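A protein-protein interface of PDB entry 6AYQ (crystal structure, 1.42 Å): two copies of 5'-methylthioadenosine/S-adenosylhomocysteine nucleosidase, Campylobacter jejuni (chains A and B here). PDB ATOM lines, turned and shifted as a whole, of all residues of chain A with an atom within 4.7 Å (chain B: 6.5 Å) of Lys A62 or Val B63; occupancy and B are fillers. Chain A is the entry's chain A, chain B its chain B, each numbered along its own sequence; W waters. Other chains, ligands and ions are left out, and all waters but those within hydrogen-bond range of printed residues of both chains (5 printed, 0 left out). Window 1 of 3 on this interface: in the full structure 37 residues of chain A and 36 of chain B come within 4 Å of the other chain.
Water W5 lies within hydrogen-bond range of the side-chain carboxylate of Asp A159, the side-chain amide oxygen of Gln B107, the backbone NH of Val A63 and the backbone NH of Lys A62.
Water W3 lies within hydrogen-bond range of the side-chain carboxylate of Asp B159 (2.6 Å), the side-chain amide oxygen of Gln A107 (2.8 Å), the backbone NH of Val B63 (2.9 Å) and the backbone NH of Lys B62 (3.3 Å).
Water W2 lies within hydrogen-bond range of the side-chain carboxylate of Asp B109 (2.7 Å), the side-chain carboxylate of Asp A109 (2.8 Å), the side-chain amino group of Lys A62 (3.2 Å) and the side-chain amino group of Lys B62 (3.2 Å).
Water W1 bridges O of Asp B109 (2.8 Å) and OD2 of Asp A109 (2.8 Å).
Water W4 lies within hydrogen-bond range of O of Asp A109 (2.8 Å) and OD2 of Asp B109 (2.8 Å).
N of Lys B62 lies within hydrogen-bond range of OD1 of Asp B159 (2.8 Å).
The side-chain amino group of Lys A62 sits at hydrogen-bond distance from the side-chain amide oxygen of Gln A107 (2.9 Å).
OG of Ser A65 is in hydrogen-bond range of OG of Ser A186.
N of Lys B62 is in hydrogen-bond range of O of Met B182, 3.1 Å away.
The backbone carbonyl oxygen of Lys B62 sits at hydrogen-bond distance from the side-chain hydroxyl of Thr B66, at 2.6 Å.
OD2 of Asp B109 lies within hydrogen-bond range of N of Asp B159, at 2.8 Å.
The backbone carbonyl oxygen (O) of Asp A159 lies close to the backbone carbonyl oxygen (O) of Asp B109, 3.1 Å away.
The side-chain carboxylate of Asp A159 is in salt-bridge range of the side-chain amino group of Lys B62.
The side-chain amino group (NZ) of Lys A62 lies within salt-bridge range of the side-chain carboxylate (OD2) of Asp B159 (2.7 Å).
The backbone carbonyl oxygen (O) of Asp A109 sits close to the backbone carbonyl oxygen (O) of Asp B159.
Among the printed residues, merely in contact across the chains: Asp A159 with Leu B110 (3.5 Å), Val A63 with Gln B107 (3.6 Å), Thr A66 with Thr B66 (3.6 Å), Val A63 with Thr B66 (3.6 Å), Thr A66 with Val B63 (3.7 Å), Gln A107 with Val B63 (3.7 Å), Val A63 with Ser B186 (3.7 Å), Ser A186 with Val B63 (3.7 Å), Gln A107 with Asp B159 (3.9 Å), Asp A159 with Gln B107 (3.9 Å), Lys A62 with Val B63 (3.9 Å), Thr A66 with Leu B67 (3.9 Å), Val A63 with Lys B62 (3.9 Å) and Leu A189 with Val B63 (3.99 Å).
Lys A62 touches just these residues of chain B: Val B63 and Asp B159.
Gly A158 touches none of the printed residues of chain B.
Printed residues of chain A within 4 Å of Val B63: Lys A62 (3.9 Å), Thr A66 (3.7 Å), Gln A107 (3.7 Å), Ser A186 (3.7 Å) and Leu A189 (3.99 Å).
Ser B65 touches none of the printed residues of chain A.
Printed residues of chain A within 4 Å of Leu B67: Thr A66.
Of the printed residues of chain A, Gln B107 touches Val A63 (3.6 Å) and Asp A159 (3.9 Å).
Of the printed residues of chain A, Leu B110 touches Asp A159.
The nearest printed residue of chain A that does not touch Val B63 is Val A63 (5.2 Å).
Hydrophobic or aromatic side chains of chain B that line the printed part of chain A: Val B63 and Leu B110.
Among the printed residues, 18 pairs touch across the chains.
Val A63 touches Thr B66, and with the chains exchanged Thr A66 touches Val B63.
Val A63 touches Gln B107, and with the chains exchanged Gln A107 touches Val B63.
Thr B66 touches its own counterpart, Thr A66.
Gln A107 touches Asp B159, and with the chains exchanged Asp A159 touches Gln B107.
Positions printed for both chains: 60, 61, 62, 63, 64, 65, 66, 107, 109, 159, 182 and 186.
Of the 18 pairs that touch across the chains among the printed residues, 15 have their exchanged pair printed and touching as well.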
ATOM      1  N   ILE A  60      20.006  26.839  26.487  1.00  0.00           N
ATOM      2  CA  ILE A  60      19.254  25.723  25.922  1.00  0.00           C
ATOM      3  C   ILE A  60      20.137  24.540  25.525  1.00  0.00           C
ATOM      4  O   ILE A  60      21.216  24.698  24.954  1.00  0.00           O
ATOM      5  CB  ILE A  60      18.441  26.215  24.706  1.00  0.00           C
ATOM      6  CG1 ILE A  60      17.314  27.145  25.191  1.00  0.00           C
ATOM      7  CG2 ILE A  60      17.864  25.051  23.907  1.00  0.00           C
ATOM      8  CD1 ILE A  60      16.723  27.996  24.093  1.00  0.00           C
ATOM      9  N   GLY A  61      19.640  23.329  25.813  1.00  0.00           N
ATOM     10  CA  GLY A  61      20.184  22.112  25.215  1.00  0.00           C
ATOM     11  C   GLY A  61      21.056  21.255  26.102  1.00  0.00           C
ATOM     12  O   GLY A  61      21.358  21.583  27.253  1.00  0.00           O
ATOM     13  N   LYS A  62      21.514  20.156  25.515  1.00  0.00           N
ATOM     14  CA  LYS A  62      22.186  19.108  26.265  1.00  0.00           C
ATOM     15  C   LYS A  62      23.557  19.503  26.779  1.00  0.00           C
ATOM     16  O   LYS A  62      23.879  19.237  27.936  1.00  0.00           O
ATOM     17  CB  LYS A  62      22.290  17.826  25.435  1.00  0.00           C
ATOM     18  CG  LYS A  62      20.941  17.193  25.144  1.00  0.00           C
ATOM     19  CD  LYS A  62      21.034  15.765  24.627  1.00  0.00           C
ATOM     20  CE  LYS A  62      21.959  15.623  23.438  1.00  0.00           C
ATOM     21  NZ  LYS A  62      21.939  14.256  22.869  1.00  0.00           N
ATOM     22  N   VAL A  63      24.370  20.109  25.923  1.00  0.00           N
ATOM     23  CA  VAL A  63      25.718  20.500  26.331  1.00  0.00           C
ATOM     24  C   VAL A  63      25.656  21.593  27.412  1.00  0.00           C
ATOM     25  O   VAL A  63      26.324  21.487  28.454  1.00  0.00           O
ATOM     26  CB  VAL A  63      26.562  20.956  25.121  1.00  0.00           C
ATOM     27  CG1 VAL A  63      27.878  21.590  25.557  1.00  0.00           C
ATOM     28  CG2 VAL A  63      26.812  19.786  24.172  1.00  0.00           C
ATOM     29  N   ASN A  64      24.869  22.642  27.171  1.00  0.00           N
ATOM     30  CA  ASN A  64      24.765  23.718  28.161  1.00  0.00           C
ATOM     31  C   ASN A  64      24.277  23.224  29.519  1.00  0.00           C
ATOM     32  O   ASN A  64      24.829  23.605  30.564  1.00  0.00           O
ATOM     33  CB  ASN A  64      23.838  24.823  27.662  1.00  0.00           C
ATOM     34  CG  ASN A  64      24.464  25.695  26.576  1.00  0.00           C
ATOM     35  OD1 ASN A  64      25.674  25.979  26.581  1.00  0.00           O
ATOM     36  ND2 ASN A  64      23.640  26.104  25.615  1.00  0.00           N
ATOM     37  N   SER A  65      23.246  22.375  29.518  1.00  0.00           N
ATOM     38  CA  SER A  65      22.690  21.868  30.769  1.00  0.00           C
ATOM     39  C   SER A  65      23.617  20.875  31.462  1.00  0.00           C
ATOM     40  O   SER A  65      23.732  20.899  32.684  1.00  0.00           O
ATOM     41  CB  SER A  65      21.297  21.260  30.547  1.00  0.00           C
ATOM     42  OG  SER A  65      21.334  20.145  29.667  1.00  0.00           O
ATOM     43  N   THR A  66      24.351  20.070  30.693  1.00  0.00           N
ATOM     44  CA  THR A  66      25.376  19.189  31.286  1.00  0.00           C
ATOM     45  C   THR A  66      26.450  20.008  32.001  1.00  0.00           C
ATOM     46  O   THR A  66      26.829  19.712  33.141  1.00  0.00           O
ATOM     47  CB  THR A  66      26.039  18.326  30.199  1.00  0.00           C
ATOM     48  OG1 THR A  66      25.040  17.535  29.539  1.00  0.00           O
ATOM     49  CG2 THR A  66      27.110  17.394  30.761  1.00  0.00           C
ATOM     50  N   GLN A 107      18.022   9.934  26.002  1.00  0.00           N
ATOM     51  CA  GLN A 107      18.413  10.831  24.897  1.00  0.00           C
ATOM     52  C   GLN A 107      17.979  10.211  23.571  1.00  0.00           C
ATOM     53  O   GLN A 107      18.627   9.274  23.079  1.00  0.00           O
ATOM     54  CB  GLN A 107      19.920  11.069  24.868  1.00  0.00           C
ATOM     55  CG  GLN A 107      20.441  11.902  26.020  1.00  0.00           C
ATOM     56  CD  GLN A 107      21.947  11.977  26.013  1.00  0.00           C
ATOM     57  OE1 GLN A 107      22.550  12.463  25.055  1.00  0.00           O
ATOM     58  NE2 GLN A 107      22.573  11.466  27.066  1.00  0.00           N
ATOM     59  N   ASP A 109      18.104  11.374  20.555  1.00  0.00           N
ATOM     60  CA  ASP A 109      18.964  11.712  19.426  1.00  0.00           C
ATOM     61  C   ASP A 109      20.407  11.230  19.558  1.00  0.00           C
ATOM     62  O   ASP A 109      21.266  11.650  18.794  1.00  0.00           O
ATOM     63  CB  ASP A 109      18.912  13.229  19.135  1.00  0.00           C
ATOM     64  CG  ASP A 109      19.450  14.081  20.262  1.00  0.00           C
ATOM     65  OD1 ASP A 109      19.703  13.566  21.363  1.00  0.00           O
ATOM     66  OD2 ASP A 109      19.575  15.302  20.022  1.00  0.00           O
ATOM     67  N   THR A 157      14.716  13.344  25.869  1.00  0.00           N
ATOM     68  CA  THR A 157      15.533  14.545  25.717  1.00  0.00           C
ATOM     69  C   THR A 157      16.343  14.498  24.428  1.00  0.00           C
ATOM     70  O   THR A 157      16.895  13.462  24.068  1.00  0.00           O
ATOM     71  CB  THR A 157      16.502  14.652  26.917  1.00  0.00           C
ATOM     72  OG1 THR A 157      15.756  14.858  28.119  1.00  0.00           O
ATOM     73  CG2 THR A 157      17.505  15.786  26.741  1.00  0.00           C
ATOM     74  N   GLY A 158      16.454  15.642  23.747  1.00  0.00           N
ATOM     75  CA  GLY A 158      17.312  15.742  22.573  1.00  0.00           C
ATOM     76  C   GLY A 158      17.500  17.203  22.226  1.00  0.00           C
ATOM     77  O   GLY A 158      16.856  18.070  22.824  1.00  0.00           O
ATOM     78  N   ASP A 159      18.367  17.480  21.266  1.00  0.00           N
ATOM     79  CA  ASP A 159      18.758  18.865  20.957  1.00  0.00           C
ATOM     80  C   ASP A 159      17.936  19.505  19.838  1.00  0.00           C
ATOM     81  O   ASP A 159      18.414  20.441  19.185  1.00  0.00           O
ATOM     82  CB  ASP A 159      20.273  18.942  20.703  1.00  0.00           C
ATOM     83  CG  ASP A 159      21.078  19.277  21.964  1.00  0.00           C
ATOM     84  OD1 ASP A 159      20.501  19.772  22.948  1.00  0.00           O
ATOM     85  OD2 ASP A 159      22.305  19.044  21.955  1.00  0.00           O
ATOM     86  N   MET A 182      14.955  19.434  26.179  1.00  0.00           N
ATOM     87  CA  MET A 182      16.308  19.480  25.620  1.00  0.00           C
ATOM     88  C   MET A 182      17.412  19.458  26.680  1.00  0.00           C
ATOM     89  O   MET A 182      18.574  19.684  26.353  1.00  0.00           O
ATOM     90  CB  MET A 182      16.435  20.731  24.706  1.00  0.00           C
ATOM     91  CG  MET A 182      15.390  20.764  23.597  1.00  0.00           C
ATOM     92  SD  MET A 182      15.332  22.296  22.635  1.00  0.00           S
ATOM     93  CE  MET A 182      16.909  22.197  21.837  1.00  0.00           C
ATOM     94  N   SER A 186      20.313  14.818  30.156  1.00  0.00           N
ATOM     95  CA  SER A 186      21.708  15.206  30.331  1.00  0.00           C
ATOM     96  C   SER A 186      21.967  15.623  31.777  1.00  0.00           C
ATOM     97  O   SER A 186      22.949  15.199  32.395  1.00  0.00           O
ATOM     98  CB  SER A 186      22.052  16.317  29.342  1.00  0.00           C
ATOM     99  OG  SER A 186      20.986  17.238  29.185  1.00  0.00           O
ATOM    100  N   LEU A 189      21.861  12.494  33.932  1.00  0.00           N
ATOM    101  CA  LEU A 189      23.073  11.712  33.750  1.00  0.00           C
ATOM    102  C   LEU A 189      24.206  12.261  34.612  1.00  0.00           C
ATOM    103  O   LEU A 189      24.893  11.508  35.298  1.00  0.00           O
ATOM    104  CB  LEU A 189      23.464  11.667  32.268  1.00  0.00           C
ATOM    105  CG  LEU A 189      24.694  10.831  31.890  1.00  0.00           C
ATOM    106  CD1 LEU A 189      24.571  10.325  30.457  1.00  0.00           C
ATOM    107  CD2 LEU A 189      26.017  11.563  32.099  1.00  0.00           C
ATOM    108  N   ILE B  60      31.166   7.833  24.488  1.00  0.00           N
ATOM    109  CA  ILE B  60      30.815   8.475  23.217  1.00  0.00           C
ATOM    110  C   ILE B  60      29.804   9.597  23.387  1.00  0.00           C
ATOM    111  O   ILE B  60      28.848   9.482  24.146  1.00  0.00           O
ATOM    112  CB  ILE B  60      30.293   7.419  22.215  1.00  0.00           C
ATOM    113  CG1 ILE B  60      31.453   6.487  21.828  1.00  0.00           C
ATOM    114  CG2 ILE B  60      29.678   8.054  20.973  1.00  0.00           C
ATOM    115  CD1 ILE B  60      31.012   5.187  21.223  1.00  0.00           C
ATOM    116  N   GLY B  61      30.026  10.679  22.647  1.00  0.00           N
ATOM    117  CA  GLY B  61      28.984  11.682  22.436  1.00  0.00           C
ATOM    118  C   GLY B  61      29.115  12.961  23.232  1.00  0.00           C
ATOM    119  O   GLY B  61      30.049  13.158  24.014  1.00  0.00           O
ATOM    120  N   LYS B  62      28.145  13.841  23.017  1.00  0.00           N
ATOM    121  CA  LYS B  62      28.275  15.230  23.466  1.00  0.00           C
ATOM    122  C   LYS B  62      28.165  15.370  24.978  1.00  0.00           C
ATOM    123  O   LYS B  62      28.944  16.101  25.593  1.00  0.00           O
ATOM    124  CB  LYS B  62      27.226  16.121  22.795  1.00  0.00           C
ATOM    125  CG  LYS B  62      27.450  16.309  21.298  1.00  0.00           C
ATOM    126  CD  LYS B  62      26.642  17.463  20.742  1.00  0.00           C
ATOM    127  CE  LYS B  62      25.154  17.285  20.972  1.00  0.00           C
ATOM    128  NZ  LYS B  62      24.364  18.364  20.309  1.00  0.00           N
ATOM    129  N   VAL B  63      27.190  14.690  25.573  1.00  0.00           N
ATOM    130  CA  VAL B  63      26.985  14.778  27.022  1.00  0.00           C
ATOM    131  C   VAL B  63      28.179  14.176  27.761  1.00  0.00           C
ATOM    132  O   VAL B  63      28.712  14.789  28.691  1.00  0.00           O
ATOM    133  CB  VAL B  63      25.652  14.115  27.431  1.00  0.00           C
ATOM    134  CG1 VAL B  63      25.520  13.957  28.947  1.00  0.00           C
ATOM    135  CG2 VAL B  63      24.504  14.956  26.901  1.00  0.00           C
ATOM    136  N   ASN B  64      28.601  12.987  27.356  1.00  0.00           N
ATOM    137  CA  ASN B  64      29.716  12.313  28.044  1.00  0.00           C
ATOM    138  C   ASN B  64      30.996  13.148  27.971  1.00  0.00           C
ATOM    139  O   ASN B  64      31.710  13.322  28.984  1.00  0.00           O
ATOM    140  CB  ASN B  64      29.965  10.931  27.437  1.00  0.00           C
ATOM    141  CG  ASN B  64      28.950   9.899  27.874  1.00  0.00           C
ATOM    142  OD1 ASN B  64      28.460   9.919  29.019  1.00  0.00           O
ATOM    143  ND2 ASN B  64      28.646   8.967  26.977  1.00  0.00           N
ATOM    144  N   SER B  65      31.274  13.701  26.788  1.00  0.00           N
ATOM    145  CA  SER B  65      32.496  14.465  26.602  1.00  0.00           C
ATOM    146  C   SER B  65      32.450  15.809  27.354  1.00  0.00           C
ATOM    147  O   SER B  65      33.471  16.240  27.918  1.00  0.00           O
ATOM    148  CB  SER B  65      32.791  14.639  25.109  1.00  0.00           C
ATOM    149  OG  SER B  65      31.785  15.347  24.431  1.00  0.00           O
ATOM    150  N   THR B  66      31.277  16.453  27.383  1.00  0.00           N
ATOM    151  CA  THR B  66      31.067  17.654  28.174  1.00  0.00           C
ATOM    152  C   THR B  66      31.367  17.391  29.645  1.00  0.00           C
ATOM    153  O   THR B  66      32.075  18.178  30.284  1.00  0.00           O
ATOM    154  CB  THR B  66      29.619  18.170  28.028  1.00  0.00           C
ATOM    155  OG1 THR B  66      29.359  18.469  26.654  1.00  0.00           O
ATOM    156  CG2 THR B  66      29.374  19.427  28.860  1.00  0.00           C
ATOM    157  N   LEU B  67      30.832  16.287  30.175  1.00  0.00           N
ATOM    158  CA  LEU B  67      31.037  15.959  31.580  1.00  0.00           C
ATOM    159  C   LEU B  67      32.506  15.730  31.894  1.00  0.00           C
ATOM    160  O   LEU B  67      33.023  16.279  32.876  1.00  0.00           O
ATOM    161  CB  LEU B  67      30.214  14.740  31.981  1.00  0.00           C
ATOM    162  CG  LEU B  67      30.370  14.255  33.429  1.00  0.00           C
ATOM    163  CD1 LEU B  67      30.123  15.351  34.459  1.00  0.00           C
ATOM    164  CD2 LEU B  67      29.458  13.064  33.674  1.00  0.00           C
ATOM    165  N   SER B  68      33.188  14.946  31.064  1.00  0.00           N
ATOM    166  CA  SER B  68      34.605  14.661  31.317  1.00  0.00           C
ATOM    167  C   SER B  68      35.448  15.931  31.255  1.00  0.00           C
ATOM    168  O   SER B  68      36.324  16.129  32.106  1.00  0.00           O
ATOM    169  CB  SER B  68      35.170  13.616  30.352  1.00  0.00           C
ATOM    170  OG  SER B  68      34.746  12.329  30.695  1.00  0.00           O
ATOM    171  N   GLN B 107      27.803  22.496  16.526  1.00  0.00           N
ATOM    172  CA  GLN B 107      26.904  21.365  16.767  1.00  0.00           C
ATOM    173  C   GLN B 107      25.833  21.345  15.670  1.00  0.00           C
ATOM    174  O   GLN B 107      24.892  22.144  15.700  1.00  0.00           O
ATOM    175  CB  GLN B 107      26.262  21.462  18.138  1.00  0.00           C
ATOM    176  CG  GLN B 107      27.224  21.309  19.301  1.00  0.00           C
ATOM    177  CD  GLN B 107      26.537  21.569  20.625  1.00  0.00           C
ATOM    178  OE1 GLN B 107      25.598  20.851  20.985  1.00  0.00           O
ATOM    179  NE2 GLN B 107      27.011  22.561  21.368  1.00  0.00           N
ATOM    180  N   ASP B 109      23.453  19.286  15.143  1.00  0.00           N
ATOM    181  CA  ASP B 109      22.162  18.753  15.593  1.00  0.00           C
ATOM    182  C   ASP B 109      21.540  19.556  16.719  1.00  0.00           C
ATOM    183  O   ASP B 109      20.591  19.098  17.348  1.00  0.00           O
ATOM    184  CB  ASP B 109      22.314  17.280  15.992  1.00  0.00           C
ATOM    185  CG  ASP B 109      23.254  17.061  17.163  1.00  0.00           C
ATOM    186  OD1 ASP B 109      23.978  17.995  17.574  1.00  0.00           O
ATOM    187  OD2 ASP B 109      23.262  15.895  17.658  1.00  0.00           O
ATOM    188  N   LEU B 110      22.055  20.755  16.963  1.00  0.00           N
ATOM    189  CA  LEU B 110      21.459  21.681  17.921  1.00  0.00           C
ATOM    190  C   LEU B 110      20.529  22.575  17.119  1.00  0.00           C
ATOM    191  O   LEU B 110      20.995  23.429  16.345  1.00  0.00           O
ATOM    192  CB  LEU B 110      22.538  22.479  18.648  1.00  0.00           C
ATOM    193  CG  LEU B 110      22.079  23.441  19.740  1.00  0.00           C
ATOM    194  CD1 LEU B 110      21.236  22.776  20.824  1.00  0.00           C
ATOM    195  CD2 LEU B 110      23.308  24.087  20.345  1.00  0.00           C
ATOM    196  N   ASP B 159      25.405  14.083  17.778  1.00  0.00           N
ATOM    197  CA  ASP B 159      25.255  12.794  18.470  1.00  0.00           C
ATOM    198  C   ASP B 159      24.800  11.655  17.568  1.00  0.00           C
ATOM    199  O   ASP B 159      24.240  10.668  18.066  1.00  0.00           O
ATOM    200  CB  ASP B 159      24.342  12.954  19.693  1.00  0.00           C
ATOM    201  CG  ASP B 159      25.106  13.291  20.965  1.00  0.00           C
ATOM    202  OD1 ASP B 159      26.340  13.079  21.006  1.00  0.00           O
ATOM    203  OD2 ASP B 159      24.461  13.743  21.938  1.00  0.00           O
ATOM    204  N   MET B 182      31.645  13.348  17.366  1.00  0.00           N
ATOM    205  CA  MET B 182      30.565  13.396  18.342  1.00  0.00           C
ATOM    206  C   MET B 182      30.940  14.039  19.677  1.00  0.00           C
ATOM    207  O   MET B 182      30.157  13.960  20.621  1.00  0.00           O
ATOM    208  CB  MET B 182      30.015  11.973  18.541  1.00  0.00           C
ATOM    209  CG  MET B 182      29.543  11.310  17.256  1.00  0.00           C
ATOM    210  SD  MET B 182      29.047   9.590  17.455  1.00  0.00           S
ATOM    211  CE  MET B 182      27.590   9.816  18.461  1.00  0.00           C
ATOM    212  N   SER B 186      31.429  20.185  21.854  1.00  0.00           N
ATOM    213  CA  SER B 186      31.067  20.147  23.263  1.00  0.00           C
ATOM    214  C   SER B 186      32.285  20.368  24.162  1.00  0.00           C
ATOM    215  O   SER B 186      32.240  21.171  25.103  1.00  0.00           O
ATOM    216  CB  SER B 186      30.347  18.830  23.595  1.00  0.00           C
ATOM    217  OG  SER B 186      30.916  17.704  22.932  1.00  0.00           O
HETATM  218  O   HOH W   1      19.069  16.802  17.731  1.00  0.00           O
HETATM  219  O   HOH W   2      22.277  15.953  20.205  1.00  0.00           O
HETATM  220  O   HOH W   3      25.251  12.914  24.297  1.00  0.00           O
HETATM  221  O   HOH W   4      21.827  13.589  16.870  1.00  0.00           O
HETATM  222  O   HOH W   5      23.774  20.831  23.138  1.00  0.00           O
